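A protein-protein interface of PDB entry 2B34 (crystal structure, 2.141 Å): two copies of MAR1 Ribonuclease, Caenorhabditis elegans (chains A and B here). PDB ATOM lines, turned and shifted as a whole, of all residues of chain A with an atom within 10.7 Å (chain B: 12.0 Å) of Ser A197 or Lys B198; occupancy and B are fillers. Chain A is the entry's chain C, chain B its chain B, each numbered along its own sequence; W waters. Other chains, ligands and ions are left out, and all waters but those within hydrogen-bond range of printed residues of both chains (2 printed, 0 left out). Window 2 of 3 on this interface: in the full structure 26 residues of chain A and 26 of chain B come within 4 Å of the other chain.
The backbone carbonyl oxygen of Leu B196 sits at hydrogen-bond distance from the backbone NH of Leu A196 (2.7 Å). OG of Ser B197 lies close to O of Gly A192, 3.5 Å away. The backbone carbonyl oxygen (O) of Val A194 sits at hydrogen-bond distance from the side-chain hydroxyl (OG) of Ser B197, 2.6 Å away. N of Lys B198 sits at hydrogen-bond distance from O of Val A194, 3.0 Å away. OG of Ser A197 sits at hydrogen-bond distance from NZ of Lys B198 (3.3 Å).
Among the printed residues, pairs that only touch across the chains: Pro A195 with Leu B196, Pro A195 with Lys B198, Leu A196 with Lys B198, Leu A196 with Ser B197, Pro A195 with Pro B195 and Leu A193 with Ser B197.
Ser A197 touches just one residue of chain B: Lys B198 (3.3 Å). Of chain A, only Val A194, Pro A195, Leu A196 and Ser A197 come within 4 Å of Lys B198. No residue of chain B comes within 4 Å of Asp A190. Of chain B, only Ser B197 comes within 4 Å of Gly A192. Of chain B, only Ser B197 (2.6 Å) and Lys B198 (3.0 Å) come within 4 Å of Val A194. Leu A196 touches just these residues of chain B: Leu B196, Ser B197 and Lys B198. No residue of chain B comes within 4 Å of Leu A199. No residue of chain A comes within 4 Å of Leu B199. Printed residues of chain A within 4 Å of Pro B195: Pro A195. Printed residues of chain A within 4 Å of Leu B196: Pro A195 and Leu A196. Of the printed residues of chain B, Leu A193 touches Ser B197. The nearest residue of chain B that does not touch Ser A197 is Leu B196 (6.0 Å).
Printed residues of chain B that touch a printed residue of chain A: Pro B195, Leu B196, Ser B197 and Lys B198. Hydrophobic or aromatic side chains of chain B within 4 Å of the printed part of chain A: Pro B195 and Leu B196. Among the printed residues, 11 pairs touch across the chains. Among the printed residues, no Asp or Glu carboxylate lies within 4 Å of a Lys or Arg side-chain nitrogen of the other chain.
Val A194 touches Lys B198, but with the chains exchanged Lys A198 does not touch Val B194 (13.3 Å). Pro A195 touches Leu B196, but with the chains exchanged Leu A196 does not touch Pro B195 (5.7 Å). Leu B196 touches its own counterpart, Leu A196. Leu A196 touches Ser B197, but with the chains exchanged Ser A197 does not touch Leu B196 (6.0 Å). 6 positions are printed for both chains. Of the 11 pairs that touch across the chains among the printed residues, 2 have their exchanged pair printed and touching as well.
Water W2 lies within hydrogen-bond range of OG of Ser B197 (2.8 Å), N of Val A194 (3.2 Å) and N of Leu A193 (3.3 Å). Water W1 bridges the backbone carbonyl oxygen (O) of Pro B195 (2.8 Å) and the backbone carbonyl oxygen (O) of Gly A192 (3.1 Å).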
ATOM      1  N   TYR A  32     -26.730 -24.724 -15.049  1.00  0.00           N
ATOM      2  CA  TYR A  32     -28.095 -24.896 -15.563  1.00  0.00           C
ATOM      3  C   TYR A  32     -28.401 -26.324 -16.014  1.00  0.00           C
ATOM      4  O   TYR A  32     -29.094 -26.527 -17.015  1.00  0.00           O
ATOM      5  CB  TYR A  32     -28.380 -23.920 -16.714  1.00  0.00           C
ATOM      6  CG  TYR A  32     -28.232 -22.462 -16.342  1.00  0.00           C
ATOM      7  CD1 TYR A  32     -29.216 -21.816 -15.595  1.00  0.00           C
ATOM      8  CD2 TYR A  32     -27.112 -21.729 -16.739  1.00  0.00           C
ATOM      9  CE1 TYR A  32     -29.095 -20.482 -15.252  1.00  0.00           C
ATOM     10  CE2 TYR A  32     -26.979 -20.383 -16.394  1.00  0.00           C
ATOM     11  CZ  TYR A  32     -27.981 -19.772 -15.653  1.00  0.00           C
ATOM     12  OH  TYR A  32     -27.879 -18.449 -15.301  1.00  0.00           O
ATOM     13  N   ALA A 188     -38.829 -22.320 -23.114  1.00  0.00           N
ATOM     14  CA  ALA A 188     -37.738 -23.090 -22.518  1.00  0.00           C
ATOM     15  C   ALA A 188     -37.131 -22.283 -21.373  1.00  0.00           C
ATOM     16  O   ALA A 188     -36.987 -21.069 -21.493  1.00  0.00           O
ATOM     17  CB  ALA A 188     -36.687 -23.412 -23.558  1.00  0.00           C
ATOM     18  N   PRO A 189     -36.786 -22.952 -20.255  1.00  0.00           N
ATOM     19  CA  PRO A 189     -36.268 -22.237 -19.083  1.00  0.00           C
ATOM     20  C   PRO A 189     -34.983 -21.450 -19.368  1.00  0.00           C
ATOM     21  O   PRO A 189     -34.161 -21.876 -20.190  1.00  0.00           O
ATOM     22  CB  PRO A 189     -35.998 -23.361 -18.075  1.00  0.00           C
ATOM     23  CG  PRO A 189     -35.903 -24.615 -18.896  1.00  0.00           C
ATOM     24  CD  PRO A 189     -36.860 -24.408 -20.023  1.00  0.00           C
ATOM     25  N   ASP A 190     -34.828 -20.314 -18.692  1.00  0.00           N
ATOM     26  CA  ASP A 190     -33.649 -19.454 -18.848  1.00  0.00           C
ATOM     27  C   ASP A 190     -32.353 -20.151 -18.429  1.00  0.00           C
ATOM     28  O   ASP A 190     -32.299 -20.841 -17.408  1.00  0.00           O
ATOM     29  CB  ASP A 190     -33.799 -18.155 -18.049  1.00  0.00           C
ATOM     30  CG  ASP A 190     -34.878 -17.235 -18.600  1.00  0.00           C
ATOM     31  OD1 ASP A 190     -35.228 -17.330 -19.796  1.00  0.00           O
ATOM     32  OD2 ASP A 190     -35.371 -16.393 -17.824  1.00  0.00           O
ATOM     33  N   THR A 191     -31.317 -19.966 -19.236  1.00  0.00           N
ATOM     34  CA  THR A 191     -30.003 -20.518 -18.935  1.00  0.00           C
ATOM     35  C   THR A 191     -28.933 -19.431 -18.962  1.00  0.00           C
ATOM     36  O   THR A 191     -27.773 -19.685 -19.315  1.00  0.00           O
ATOM     37  CB  THR A 191     -29.622 -21.676 -19.882  1.00  0.00           C
ATOM     38  OG1 THR A 191     -29.623 -21.217 -21.236  1.00  0.00           O
ATOM     39  CG2 THR A 191     -30.590 -22.840 -19.731  1.00  0.00           C
ATOM     40  N   GLY A 192     -29.341 -18.222 -18.585  1.00  0.00           N
ATOM     41  CA  GLY A 192     -28.429 -17.095 -18.410  1.00  0.00           C
ATOM     42  C   GLY A 192     -27.691 -16.634 -19.654  1.00  0.00           C
ATOM     43  O   GLY A 192     -26.557 -16.160 -19.563  1.00  0.00           O
ATOM     44  N   LEU A 193     -28.339 -16.753 -20.811  1.00  0.00           N
ATOM     45  CA  LEU A 193     -27.697 -16.440 -22.098  1.00  0.00           C
ATOM     46  C   LEU A 193     -27.875 -15.000 -22.582  1.00  0.00           C
ATOM     47  O   LEU A 193     -27.213 -14.578 -23.526  1.00  0.00           O
ATOM     48  CB  LEU A 193     -28.167 -17.413 -23.184  1.00  0.00           C
ATOM     49  CG  LEU A 193     -27.744 -18.875 -23.025  1.00  0.00           C
ATOM     50  CD1 LEU A 193     -28.502 -19.749 -24.014  1.00  0.00           C
ATOM     51  CD2 LEU A 193     -26.237 -19.034 -23.189  1.00  0.00           C
ATOM     52  N   VAL A 194     -28.771 -14.257 -21.943  1.00  0.00           N
ATOM     53  CA  VAL A 194     -29.071 -12.889 -22.359  1.00  0.00           C
ATOM     54  C   VAL A 194     -28.575 -11.932 -21.277  1.00  0.00           C
ATOM     55  O   VAL A 194     -29.007 -12.029 -20.128  1.00  0.00           O
ATOM     56  CB  VAL A 194     -30.596 -12.673 -22.598  1.00  0.00           C
ATOM     57  CG1 VAL A 194     -30.877 -11.284 -23.199  1.00  0.00           C
ATOM     58  CG2 VAL A 194     -31.158 -13.760 -23.492  1.00  0.00           C
ATOM     59  N   PRO A 195     -27.662 -11.012 -21.642  1.00  0.00           N
ATOM     60  CA  PRO A 195     -27.108 -10.046 -20.690  1.00  0.00           C
ATOM     61  C   PRO A 195     -28.185  -9.155 -20.079  1.00  0.00           C
ATOM     62  O   PRO A 195     -29.135  -8.783 -20.771  1.00  0.00           O
ATOM     63  CB  PRO A 195     -26.178  -9.194 -21.557  1.00  0.00           C
ATOM     64  CG  PRO A 195     -25.868 -10.047 -22.746  1.00  0.00           C
ATOM     65  CD  PRO A 195     -27.108 -10.826 -22.997  1.00  0.00           C
ATOM     66  N   LEU A 196     -28.046  -8.853 -18.785  1.00  0.00           N
ATOM     67  CA  LEU A 196     -28.805  -7.782 -18.146  1.00  0.00           C
ATOM     68  C   LEU A 196     -28.546  -6.496 -18.926  1.00  0.00           C
ATOM     69  O   LEU A 196     -27.402  -6.182 -19.248  1.00  0.00           O
ATOM     70  CB  LEU A 196     -28.374  -7.588 -16.685  1.00  0.00           C
ATOM     71  CG  LEU A 196     -29.084  -8.296 -15.523  1.00  0.00           C
ATOM     72  CD1 LEU A 196     -28.349  -8.010 -14.219  1.00  0.00           C
ATOM     73  CD2 LEU A 196     -30.528  -7.858 -15.392  1.00  0.00           C
ATOM     74  N   SER A 197     -29.611  -5.768 -19.235  1.00  0.00           N
ATOM     75  CA  SER A 197     -29.520  -4.594 -20.087  1.00  0.00           C
ATOM     76  C   SER A 197     -29.457  -3.309 -19.276  1.00  0.00           C
ATOM     77  O   SER A 197     -29.869  -3.282 -18.114  1.00  0.00           O
ATOM     78  CB  SER A 197     -30.712  -4.545 -21.040  1.00  0.00           C
ATOM     79  OG  SER A 197     -31.907  -4.274 -20.333  1.00  0.00           O
ATOM     80  N   LYS A 198     -28.945  -2.248 -19.895  1.00  0.00           N
ATOM     81  CA  LYS A 198     -28.950  -0.925 -19.277  1.00  0.00           C
ATOM     82  C   LYS A 198     -29.909   0.039 -19.976  1.00  0.00           C
ATOM     83  O   LYS A 198     -30.260  -0.161 -21.143  1.00  0.00           O
ATOM     84  CB  LYS A 198     -27.538  -0.342 -19.220  1.00  0.00           C
ATOM     85  CG  LYS A 198     -26.912   0.015 -20.558  1.00  0.00           C
ATOM     86  CD  LYS A 198     -25.594   0.720 -20.295  1.00  0.00           C
ATOM     87  CE  LYS A 198     -24.952   1.252 -21.556  1.00  0.00           C
ATOM     88  NZ  LYS A 198     -23.749   2.030 -21.181  1.00  0.00           N
ATOM     89  N   LEU A 199     -30.332   1.074 -19.246  1.00  0.00           N
ATOM     90  CA  LEU A 199     -31.210   2.118 -19.784  1.00  0.00           C
ATOM     91  C   LEU A 199     -30.435   3.287 -20.375  1.00  0.00           C
ATOM     92  O   LEU A 199     -29.338   3.628 -19.924  1.00  0.00           O
ATOM     93  CB  LEU A 199     -32.171   2.647 -18.710  1.00  0.00           C
ATOM     94  CG  LEU A 199     -33.628   2.176 -18.697  1.00  0.00           C
ATOM     95  CD1 LEU A 199     -34.457   3.135 -17.856  1.00  0.00           C
ATOM     96  CD2 LEU A 199     -34.222   2.068 -20.093  1.00  0.00           C
ATOM     97  OXT LEU A 199     -30.909   3.924 -21.317  1.00  0.00           O
ATOM     98  N   VAL B 194     -17.953 -13.186 -19.041  1.00  0.00           N
ATOM     99  CA  VAL B 194     -19.338 -13.559 -19.334  1.00  0.00           C
ATOM    100  C   VAL B 194     -20.289 -12.458 -18.861  1.00  0.00           C
ATOM    101  O   VAL B 194     -20.219 -12.038 -17.707  1.00  0.00           O
ATOM    102  CB  VAL B 194     -19.731 -14.911 -18.674  1.00  0.00           C
ATOM    103  CG1 VAL B 194     -21.154 -15.314 -19.061  1.00  0.00           C
ATOM    104  CG2 VAL B 194     -18.743 -16.006 -19.057  1.00  0.00           C
ATOM    105  N   PRO B 195     -21.182 -11.983 -19.751  1.00  0.00           N
ATOM    106  CA  PRO B 195     -22.143 -10.976 -19.300  1.00  0.00           C
ATOM    107  C   PRO B 195     -23.058 -11.521 -18.205  1.00  0.00           C
ATOM    108  O   PRO B 195     -23.503 -12.665 -18.295  1.00  0.00           O
ATOM    109  CB  PRO B 195     -22.946 -10.662 -20.565  1.00  0.00           C
ATOM    110  CG  PRO B 195     -22.078 -11.113 -21.703  1.00  0.00           C
ATOM    111  CD  PRO B 195     -21.357 -12.313 -21.176  1.00  0.00           C
ATOM    112  N   LEU B 196     -23.293 -10.724 -17.163  1.00  0.00           N
ATOM    113  CA  LEU B 196     -24.289 -11.055 -16.138  1.00  0.00           C
ATOM    114  C   LEU B 196     -25.661 -11.072 -16.810  1.00  0.00           C
ATOM    115  O   LEU B 196     -25.966 -10.193 -17.619  1.00  0.00           O
ATOM    116  CB  LEU B 196     -24.270 -10.026 -15.000  1.00  0.00           C
ATOM    117  CG  LEU B 196     -24.758 -10.453 -13.602  1.00  0.00           C
ATOM    118  CD1 LEU B 196     -24.513  -9.353 -12.578  1.00  0.00           C
ATOM    119  CD2 LEU B 196     -26.220 -10.858 -13.570  1.00  0.00           C
ATOM    120  N   SER B 197     -26.482 -12.066 -16.472  1.00  0.00           N
ATOM    121  CA  SER B 197     -27.726 -12.309 -17.197  1.00  0.00           C
ATOM    122  C   SER B 197     -29.015 -11.860 -16.506  1.00  0.00           C
ATOM    123  O   SER B 197     -29.136 -11.928 -15.281  1.00  0.00           O
ATOM    124  CB  SER B 197     -27.845 -13.783 -17.573  1.00  0.00           C
ATOM    125  OG  SER B 197     -28.972 -13.981 -18.412  1.00  0.00           O
ATOM    126  N   LYS B 198     -29.981 -11.441 -17.326  1.00  0.00           N
ATOM    127  CA  LYS B 198     -31.287 -10.976 -16.858  1.00  0.00           C
ATOM    128  C   LYS B 198     -32.243 -12.110 -16.504  1.00  0.00           C
ATOM    129  O   LYS B 198     -32.359 -13.099 -17.241  1.00  0.00           O
ATOM    130  CB  LYS B 198     -31.937 -10.037 -17.882  1.00  0.00           C
ATOM    131  CG  LYS B 198     -32.197 -10.641 -19.266  1.00  0.00           C
ATOM    132  CD  LYS B 198     -33.156  -9.784 -20.099  1.00  0.00           C
ATOM    133  CE  LYS B 198     -32.528  -8.463 -20.551  1.00  0.00           C
ATOM    134  NZ  LYS B 198     -32.664  -7.368 -19.545  1.00  0.00           N
ATOM    135  N   LEU B 199     -32.934 -11.946 -15.374  1.00  0.00           N
ATOM    136  CA  LEU B 199     -33.876 -12.949 -14.869  1.00  0.00           C
ATOM    137  C   LEU B 199     -35.184 -12.949 -15.669  1.00  0.00           C
ATOM    138  O   LEU B 199     -36.231 -13.401 -15.196  1.00  0.00           O
ATOM    139  CB  LEU B 199     -34.158 -12.716 -13.374  1.00  0.00           C
ATOM    140  CG  LEU B 199     -32.987 -12.575 -12.386  1.00  0.00           C
ATOM    141  CD1 LEU B 199     -33.455 -11.913 -11.086  1.00  0.00           C
ATOM    142  CD2 LEU B 199     -32.312 -13.921 -12.103  1.00  0.00           C
ATOM    143  OXT LEU B 199     -35.234 -12.502 -16.820  1.00  0.00           O
HETATM  144  O   HOH W   1     -25.283 -13.477 -20.322  1.00  0.00           O
HETATM  145  O   HOH W   2     -31.047 -15.195 -19.869  1.00  0.00           O
